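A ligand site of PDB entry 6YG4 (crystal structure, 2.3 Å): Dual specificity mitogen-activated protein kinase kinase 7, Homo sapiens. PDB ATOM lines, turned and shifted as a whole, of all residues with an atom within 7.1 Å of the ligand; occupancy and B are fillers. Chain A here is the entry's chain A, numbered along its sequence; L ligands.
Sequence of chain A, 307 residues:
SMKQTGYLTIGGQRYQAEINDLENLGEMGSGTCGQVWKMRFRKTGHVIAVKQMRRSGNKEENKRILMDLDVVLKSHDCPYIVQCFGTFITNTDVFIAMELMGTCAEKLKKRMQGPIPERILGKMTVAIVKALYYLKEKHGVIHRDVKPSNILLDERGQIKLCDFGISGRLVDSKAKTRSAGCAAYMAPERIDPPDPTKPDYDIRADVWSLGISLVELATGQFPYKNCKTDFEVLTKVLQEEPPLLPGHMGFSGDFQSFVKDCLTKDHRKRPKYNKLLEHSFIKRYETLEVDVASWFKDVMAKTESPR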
ATOM      1  N   MET A  28      27.600  -3.668 -16.223  1.00  0.00           N
ATOM      2  CA  MET A  28      27.315  -5.089 -16.512  1.00  0.00           C
ATOM      3  C   MET A  28      28.516  -5.965 -16.087  1.00  0.00           C
ATOM      4  O   MET A  28      28.301  -6.890 -15.297  1.00  0.00           O
ATOM      5  CB  MET A  28      27.029  -5.279 -18.000  1.00  0.00           C
ATOM      6  CG  MET A  28      25.879  -6.216 -18.294  1.00  0.00           C
ATOM      7  SD  MET A  28      24.284  -5.386 -18.340  1.00  0.00           S
ATOM      8  CE  MET A  28      24.303  -4.714 -19.993  1.00  0.00           C
ATOM      9  N   GLY A  29      29.733  -5.678 -16.597  1.00  0.00           N
ATOM     10  CA  GLY A  29      30.953  -6.494 -16.398  1.00  0.00           C
ATOM     11  C   GLY A  29      31.811  -6.535 -17.663  1.00  0.00           C
ATOM     12  O   GLY A  29      31.963  -7.653 -18.227  1.00  0.00           O
ATOM     13  N   VAL A  36      30.800  -1.730 -20.030  1.00  0.00           N
ATOM     14  CA  VAL A  36      29.429  -1.799 -20.641  1.00  0.00           C
ATOM     15  C   VAL A  36      28.361  -1.527 -19.560  1.00  0.00           C
ATOM     16  O   VAL A  36      28.309  -2.262 -18.547  1.00  0.00           O
ATOM     17  CB  VAL A  36      29.189  -3.128 -21.379  1.00  0.00           C
ATOM     18  CG1 VAL A  36      28.986  -4.288 -20.448  1.00  0.00           C
ATOM     19  CG2 VAL A  36      28.035  -3.017 -22.348  1.00  0.00           C
ATOM     20  N   ILE A  48      19.030  -1.173 -23.050  1.00  0.00           N
ATOM     21  CA  ILE A  48      20.156  -1.434 -23.983  1.00  0.00           C
ATOM     22  C   ILE A  48      21.463  -1.505 -23.195  1.00  0.00           C
ATOM     23  O   ILE A  48      21.481  -1.146 -22.018  1.00  0.00           O
ATOM     24  CB  ILE A  48      20.264  -0.333 -25.068  1.00  0.00           C
ATOM     25  CG1 ILE A  48      20.739   0.982 -24.438  1.00  0.00           C
ATOM     26  CG2 ILE A  48      18.954  -0.198 -25.822  1.00  0.00           C
ATOM     27  CD1 ILE A  48      20.659   2.180 -25.336  1.00  0.00           C
ATOM     28  N   ALA A  49      22.521  -1.897 -23.886  1.00  0.00           N
ATOM     29  CA  ALA A  49      23.893  -1.930 -23.387  1.00  0.00           C
ATOM     30  C   ALA A  49      24.590  -0.752 -23.998  1.00  0.00           C
ATOM     31  O   ALA A  49      24.191  -0.352 -25.128  1.00  0.00           O
ATOM     32  CB  ALA A  49      24.546  -3.233 -23.776  1.00  0.00           C
ATOM     33  N   VAL A  50      25.463  -0.101 -23.222  1.00  0.00           N
ATOM     34  CA  VAL A  50      26.209   1.070 -23.689  1.00  0.00           C
ATOM     35  C   VAL A  50      27.639   0.925 -23.253  1.00  0.00           C
ATOM     36  O   VAL A  50      27.855   0.801 -22.041  1.00  0.00           O
ATOM     37  CB  VAL A  50      25.612   2.364 -23.163  1.00  0.00           C
ATOM     38  CG1 VAL A  50      26.423   3.574 -23.651  1.00  0.00           C
ATOM     39  CG2 VAL A  50      24.156   2.482 -23.572  1.00  0.00           C
ATOM     40  N   LYS A  51      28.543   0.784 -24.240  1.00  0.00           N
ATOM     41  CA  LYS A  51      29.996   0.896 -24.066  1.00  0.00           C
ATOM     42  C   LYS A  51      30.365   2.371 -24.082  1.00  0.00           C
ATOM     43  O   LYS A  51      29.956   3.110 -25.029  1.00  0.00           O
ATOM     44  CB  LYS A  51      30.756   0.174 -25.191  1.00  0.00           C
ATOM     45  CG  LYS A  51      30.781  -1.341 -25.091  1.00  0.00           C
ATOM     46  CD  LYS A  51      31.906  -1.986 -25.919  1.00  0.00           C
ATOM     47  CE  LYS A  51      31.527  -2.179 -27.371  1.00  0.00           C
ATOM     48  NZ  LYS A  51      32.717  -2.414 -28.232  1.00  0.00           N
ATOM     49  N   VAL A  72      31.239  -4.411 -36.386  1.00  0.00           N
ATOM     50  CA  VAL A  72      29.845  -4.551 -35.860  1.00  0.00           C
ATOM     51  C   VAL A  72      28.886  -3.865 -36.829  1.00  0.00           C
ATOM     52  O   VAL A  72      27.816  -4.479 -37.169  1.00  0.00           O
ATOM     53  CB  VAL A  72      29.682  -3.985 -34.439  1.00  0.00           C
ATOM     54  CG1 VAL A  72      28.221  -3.926 -34.025  1.00  0.00           C
ATOM     55  CG2 VAL A  72      30.487  -4.774 -33.416  1.00  0.00           C
ATOM     56  N   VAL A  82      26.188  -9.356 -31.799  1.00  0.00           N
ATOM     57  CA  VAL A  82      25.457  -8.226 -31.162  1.00  0.00           C
ATOM     58  C   VAL A  82      25.440  -7.066 -32.145  1.00  0.00           C
ATOM     59  O   VAL A  82      26.494  -6.781 -32.736  1.00  0.00           O
ATOM     60  CB  VAL A  82      26.053  -7.799 -29.819  1.00  0.00           C
ATOM     61  CG1 VAL A  82      25.729  -8.794 -28.745  1.00  0.00           C
ATOM     62  CG2 VAL A  82      27.567  -7.558 -29.911  1.00  0.00           C
ATOM     63  N   GLN A  83      24.293  -6.412 -32.254  1.00  0.00           N
ATOM     64  CA  GLN A  83      24.069  -5.278 -33.176  1.00  0.00           C
ATOM     65  C   GLN A  83      24.204  -3.960 -32.427  1.00  0.00           C
ATOM     66  O   GLN A  83      23.923  -3.919 -31.183  1.00  0.00           O
ATOM     67  CB  GLN A  83      22.699  -5.417 -33.836  1.00  0.00           C
ATOM     68  CG  GLN A  83      22.606  -6.609 -34.796  1.00  0.00           C
ATOM     69  CD  GLN A  83      23.626  -6.590 -35.926  1.00  0.00           C
ATOM     70  OE1 GLN A  83      23.869  -5.555 -36.562  1.00  0.00           O
ATOM     71  NE2 GLN A  83      24.230  -7.733 -36.185  1.00  0.00           N
ATOM     72  N   ILE A  96      28.478   3.948 -27.226  1.00  0.00           N
ATOM     73  CA  ILE A  96      28.085   2.981 -28.282  1.00  0.00           C
ATOM     74  C   ILE A  96      26.901   2.142 -27.780  1.00  0.00           C
ATOM     75  O   ILE A  96      27.087   1.403 -26.784  1.00  0.00           O
ATOM     76  CB  ILE A  96      29.294   2.126 -28.679  1.00  0.00           C
ATOM     77  CG1 ILE A  96      30.405   3.005 -29.257  1.00  0.00           C
ATOM     78  CG2 ILE A  96      28.885   1.027 -29.646  1.00  0.00           C
ATOM     79  CD1 ILE A  96      31.746   2.339 -29.268  1.00  0.00           C
ATOM     80  N   ALA A  97      25.723   2.370 -28.369  1.00  0.00           N
ATOM     81  CA  ALA A  97      24.452   1.678 -28.055  1.00  0.00           C
ATOM     82  C   ALA A  97      24.442   0.308 -28.746  1.00  0.00           C
ATOM     83  O   ALA A  97      24.528   0.274 -29.987  1.00  0.00           O
ATOM     84  CB  ALA A  97      23.293   2.527 -28.515  1.00  0.00           C
ATOM     85  N   MET A  98      24.272  -0.761 -27.961  1.00  0.00           N
ATOM     86  CA  MET A  98      24.330  -2.170 -28.431  1.00  0.00           C
ATOM     87  C   MET A  98      23.103  -2.916 -27.919  1.00  0.00           C
ATOM     88  O   MET A  98      22.610  -2.577 -26.839  1.00  0.00           O
ATOM     89  CB  MET A  98      25.561  -2.908 -27.920  1.00  0.00           C
ATOM     90  CG  MET A  98      26.885  -2.224 -28.234  1.00  0.00           C
ATOM     91  SD  MET A  98      27.380  -2.374 -29.947  1.00  0.00           S
ATOM     92  CE  MET A  98      27.767  -4.118 -30.011  1.00  0.00           C
ATOM     93  N   GLU A  99      22.717  -3.949 -28.645  1.00  0.00           N
ATOM     94  CA  GLU A  99      21.805  -5.014 -28.210  1.00  0.00           C
ATOM     95  C   GLU A  99      22.142  -5.376 -26.770  1.00  0.00           C
ATOM     96  O   GLU A  99      23.345  -5.594 -26.502  1.00  0.00           O
ATOM     97  CB  GLU A  99      21.980  -6.221 -29.121  1.00  0.00           C
ATOM     98  CG  GLU A  99      20.702  -6.868 -29.504  1.00  0.00           C
ATOM     99  CD  GLU A  99      20.894  -8.009 -30.480  1.00  0.00           C
ATOM    100  OE1 GLU A  99      21.926  -8.018 -31.214  1.00  0.00           O
ATOM    101  OE2 GLU A  99      20.020  -8.897 -30.487  1.00  0.00           O
ATOM    102  N   LEU A 100      21.127  -5.470 -25.907  1.00  0.00           N
ATOM    103  CA  LEU A 100      21.292  -5.987 -24.533  1.00  0.00           C
ATOM    104  C   LEU A 100      21.067  -7.496 -24.532  1.00  0.00           C
ATOM    105  O   LEU A 100      20.097  -7.970 -25.131  1.00  0.00           O
ATOM    106  CB  LEU A 100      20.306  -5.295 -23.605  1.00  0.00           C
ATOM    107  CG  LEU A 100      20.347  -5.794 -22.158  1.00  0.00           C
ATOM    108  CD1 LEU A 100      21.657  -5.412 -21.514  1.00  0.00           C
ATOM    109  CD2 LEU A 100      19.180  -5.262 -21.349  1.00  0.00           C
ATOM    110  N   MET A 101      21.964  -8.220 -23.869  1.00  0.00           N
ATOM    111  CA  MET A 101      21.902  -9.683 -23.684  1.00  0.00           C
ATOM    112  C   MET A 101      21.926  -9.946 -22.190  1.00  0.00           C
ATOM    113  O   MET A 101      22.404  -9.075 -21.459  1.00  0.00           O
ATOM    114  CB  MET A 101      23.095 -10.358 -24.370  1.00  0.00           C
ATOM    115  CG  MET A 101      23.161 -10.110 -25.869  1.00  0.00           C
ATOM    116  SD  MET A 101      21.801 -10.855 -26.781  1.00  0.00           S
ATOM    117  CE  MET A 101      22.319 -12.572 -26.836  1.00  0.00           C
ATOM    118  N   GLY A 102      21.317 -11.039 -21.740  1.00  0.00           N
ATOM    119  CA  GLY A 102      21.103 -11.333 -20.322  1.00  0.00           C
ATOM    120  C   GLY A 102      22.410 -11.600 -19.598  1.00  0.00           C
ATOM    121  O   GLY A 102      22.606 -11.072 -18.518  1.00  0.00           O
ATOM    122  N   THR A 103      23.306 -12.341 -20.186  1.00  0.00           N
ATOM    123  CA  THR A 103      24.586 -12.657 -19.533  1.00  0.00           C
ATOM    124  C   THR A 103      25.513 -13.288 -20.561  1.00  0.00           C
ATOM    125  O   THR A 103      25.103 -13.433 -21.718  1.00  0.00           O
ATOM    126  CB  THR A 103      24.355 -13.557 -18.306  1.00  0.00           C
ATOM    127  OG1 THR A 103      25.593 -13.776 -17.613  1.00  0.00           O
ATOM    128  CG2 THR A 103      23.774 -14.897 -18.651  1.00  0.00           C
ATOM    129  N   CSD A 104      26.748 -13.501 -20.158  1.00  0.00           N
ATOM    130  CA  CSD A 104      27.780 -14.215 -20.924  1.00  0.00           C
ATOM    131  CB  CSD A 104      29.073 -13.430 -20.964  1.00  0.00           C
ATOM    132  SG  CSD A 104      29.562 -13.039 -19.287  1.00  0.00           S
ATOM    133  C   CSD A 104      27.936 -15.591 -20.287  1.00  0.00           C
ATOM    134  O   CSD A 104      27.445 -15.770 -19.141  1.00  0.00           O
ATOM    135  OD1 CSD A 104      30.646 -13.982 -18.978  1.00  0.00           O
ATOM    136  OD2 CSD A 104      30.100 -11.506 -19.131  1.00  0.00           O
ATOM    137  N   LYS A 107      29.873 -16.010 -16.725  1.00  0.00           N
ATOM    138  CA  LYS A 107      29.004 -15.635 -15.575  1.00  0.00           C
ATOM    139  C   LYS A 107      27.946 -16.724 -15.405  1.00  0.00           C
ATOM    140  O   LYS A 107      27.538 -16.999 -14.257  1.00  0.00           O
ATOM    141  CB  LYS A 107      28.334 -14.270 -15.794  1.00  0.00           C
ATOM    142  CG  LYS A 107      29.243 -13.056 -15.701  1.00  0.00           C
ATOM    143  CD  LYS A 107      29.747 -12.768 -14.302  1.00  0.00           C
ATOM    144  CE  LYS A 107      31.088 -12.051 -14.282  1.00  0.00           C
ATOM    145  NZ  LYS A 107      32.201 -12.941 -14.692  1.00  0.00           N
ATOM    146  N   SER A 149      33.432 -15.837 -21.858  1.00  0.00           N
ATOM    147  CA  SER A 149      33.034 -14.406 -21.620  1.00  0.00           C
ATOM    148  C   SER A 149      32.674 -13.716 -22.946  1.00  0.00           C
ATOM    149  O   SER A 149      31.908 -12.759 -22.882  1.00  0.00           O
ATOM    150  CB  SER A 149      34.079 -13.617 -20.845  1.00  0.00           C
ATOM    151  OG  SER A 149      35.360 -13.672 -21.465  1.00  0.00           O
ATOM    152  N   LEU A 152      27.390 -14.625 -25.419  1.00  0.00           N
ATOM    153  CA  LEU A 152      26.257 -13.959 -24.741  1.00  0.00           C
ATOM    154  C   LEU A 152      24.975 -14.743 -25.004  1.00  0.00           C
ATOM    155  O   LEU A 152      24.835 -15.317 -26.128  1.00  0.00           O
ATOM    156  CB  LEU A 152      26.128 -12.517 -25.239  1.00  0.00           C
ATOM    157  CG  LEU A 152      27.351 -11.629 -25.060  1.00  0.00           C
ATOM    158  CD1 LEU A 152      27.070 -10.220 -25.542  1.00  0.00           C
ATOM    159  CD2 LEU A 152      27.799 -11.598 -23.598  1.00  0.00           C
ATOM    160  N   LEU A 153      24.105 -14.779 -24.008  1.00  0.00           N
ATOM    161  CA  LEU A 153      22.725 -15.332 -24.113  1.00  0.00           C
ATOM    162  C   LEU A 153      21.727 -14.336 -23.545  1.00  0.00           C
ATOM    163  O   LEU A 153      22.102 -13.559 -22.634  1.00  0.00           O
ATOM    164  CB  LEU A 153      22.667 -16.644 -23.335  1.00  0.00           C
ATOM    165  CG  LEU A 153      23.713 -17.675 -23.736  1.00  0.00           C
ATOM    166  CD1 LEU A 153      24.994 -17.511 -22.924  1.00  0.00           C
ATOM    167  CD2 LEU A 153      23.164 -19.084 -23.574  1.00  0.00           C
ATOM    168  N   LEU A 161      27.756 -13.630 -30.483  1.00  0.00           N
ATOM    169  CA  LEU A 161      29.163 -13.324 -30.173  1.00  0.00           C
ATOM    170  C   LEU A 161      29.271 -11.873 -29.693  1.00  0.00           C
ATOM    171  O   LEU A 161      28.590 -11.005 -30.300  1.00  0.00           O
ATOM    172  CB  LEU A 161      29.977 -13.550 -31.448  1.00  0.00           C
ATOM    173  CG  LEU A 161      31.482 -13.559 -31.296  1.00  0.00           C
ATOM    174  CD1 LEU A 161      31.925 -14.640 -30.340  1.00  0.00           C
ATOM    175  CD2 LEU A 161      32.130 -13.762 -32.649  1.00  0.00           C
ATOM    176  N   CSO A 162      29.983 -11.680 -28.579  1.00  0.00           N
ATOM    177  CA  CSO A 162      30.416 -10.382 -28.016  1.00  0.00           C
ATOM    178  CB  CSO A 162      31.096 -10.616 -26.650  1.00  0.00           C
ATOM    179  SG  CSO A 162      31.729  -9.145 -25.789  1.00  0.00           S
ATOM    180  C   CSO A 162      31.347  -9.704 -29.011  1.00  0.00           C
ATOM    181  O   CSO A 162      32.058 -10.434 -29.768  1.00  0.00           O
ATOM    182  OD  CSO A 162      32.564  -9.432 -24.345  1.00  0.00           O
ATOM    183  N   ASP A 163      31.362  -8.380 -29.017  1.00  0.00           N
ATOM    184  CA  ASP A 163      32.059  -7.557 -30.041  1.00  0.00           C
ATOM    185  C   ASP A 163      33.500  -7.284 -29.593  1.00  0.00           C
ATOM    186  O   ASP A 163      34.218  -6.634 -30.369  1.00  0.00           O
ATOM    187  CB  ASP A 163      31.285  -6.275 -30.339  1.00  0.00           C
ATOM    188  CG  ASP A 163      31.437  -5.188 -29.295  1.00  0.00           C
ATOM    189  OD1 ASP A 163      31.760  -5.506 -28.125  1.00  0.00           O
ATOM    190  OD2 ASP A 163      31.209  -4.017 -29.668  1.00  0.00           O
ATOM    191  N   PHE A 164      33.950  -7.820 -28.466  1.00  0.00           N
ATOM    192  CA  PHE A 164      35.342  -7.628 -28.010  1.00  0.00           C
ATOM    193  C   PHE A 164      36.278  -8.508 -28.835  1.00  0.00           C
ATOM    194  O   PHE A 164      36.047  -9.757 -28.904  1.00  0.00           O
ATOM    195  CB  PHE A 164      35.558  -7.930 -26.526  1.00  0.00           C
ATOM    196  CG  PHE A 164      36.989  -7.757 -26.127  1.00  0.00           C
ATOM    197  CD1 PHE A 164      37.637  -6.544 -26.354  1.00  0.00           C
ATOM    198  CD2 PHE A 164      37.747  -8.822 -25.668  1.00  0.00           C
ATOM    199  CE1 PHE A 164      38.985  -6.393 -26.050  1.00  0.00           C
ATOM    200  CE2 PHE A 164      39.090  -8.666 -25.371  1.00  0.00           C
ATOM    201  CZ  PHE A 164      39.708  -7.446 -25.558  1.00  0.00           C
HETATM  202  N1  LIG L   1      25.391  -8.469 -20.937  1.00  0.00           N
HETATM  203  C1  LIG L   1      25.147  -9.090 -19.792  1.00  0.00           C
HETATM  204  N2  LIG L   1      26.279  -9.536 -19.220  1.00  0.00           N
HETATM  205  C2  LIG L   1      27.317  -9.193 -20.042  1.00  0.00           C
HETATM  206  C3  LIG L   1      26.769  -8.527 -21.080  1.00  0.00           C
HETATM  207  C4  LIG L   1      27.449  -7.916 -22.166  1.00  0.00           C
HETATM  208  C5  LIG L   1      26.976  -7.306 -23.254  1.00  0.00           C
HETATM  209  C6  LIG L   1      25.562  -7.093 -23.711  1.00  0.00           C
HETATM  210  O1  LIG L   1      24.539  -7.451 -23.137  1.00  0.00           O
HETATM  211  N3  LIG L   1      25.622  -6.436 -24.898  1.00  0.00           N
HETATM  212  C7  LIG L   1      26.939  -6.196 -25.271  1.00  0.00           C
HETATM  213  C8  LIG L   1      27.415  -5.600 -26.432  1.00  0.00           C
HETATM  214  C9  LIG L   1      28.790  -5.485 -26.595  1.00  0.00           C
HETATM  215  C10 LIG L   1      29.662  -5.943 -25.619  1.00  0.00           C
HETATM  216  C11 LIG L   1      29.181  -6.547 -24.461  1.00  0.00           C
HETATM  217  C12 LIG L   1      27.806  -6.689 -24.288  1.00  0.00           C
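The backbone carbonyl oxygen (O) of Glu 99 lies within hydrogen-bond range of a nitrogen (N3) of the ligand (2.9 Å). The backbone NH of Met 101 is in hydrogen-bond range of an oxygen (O1) of the ligand, at 2.8 Å. O of Met 101 lies within hydrogen-bond range of N1 of the ligand, at 3.1 Å.
SG of CSO 162 lies close to the backbone NH (N) of Phe 164, at 3.7 Å. N of Val 82 lies within hydrogen-bond range of O of Leu 161, at 3.3 Å. OD1 of CSD 104 sits at hydrogen-bond distance from the backbone NH of Lys 107 (3.1 Å). O of Ala 49 is in hydrogen-bond range of N of Met 98 (2.9 Å). N of Gly 102 lies within hydrogen-bond range of O of Leu 153, at 2.8 Å. The backbone NH (N) of Leu 153 sits at hydrogen-bond distance from the backbone carbonyl oxygen (O) of Thr 103, at 2.8 Å. The backbone carbonyl oxygen of Gln 83 sits at hydrogen-bond distance from the backbone NH of Glu 99 (2.8 Å). NZ of Lys 51 lies within salt-bridge range of OD2 of Asp 163 (2.6 Å).
Met 28 touches the ligand (CG to C1, 3.3 Å). CB of Ala 49 touches N3 of the ligand, 3.6 Å away. Val 82 touches the ligand (CG2 to C8, 3.995 Å). CB of Met 98 touches C8 of the ligand, 3.6 Å away. C of Leu 100 touches O1 of the ligand, 3.7 Å away. O of Gly 102 touches C1 of the ligand, at 3.5 Å. Thr 103 touches the ligand (CA to N2, 3.6 Å). CSD 104 touches the ligand (OD2 to C2, 3.7 Å). Leu 152 touches the ligand (CD1 to C5, 3.7 Å). CSO 162 touches the ligand (SG to C10, 3.8 Å). OD1 of Asp 163 touches C10 of the ligand, 3.3 Å away. 13 residues have an atom within 4 Å of the ligand: Met 28, Ala 49, Val 82, Met 98, Glu 99, Leu 100, Met 101, Gly 102, Thr 103, CSD 104, Leu 152, CSO 162 and Asp 163.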
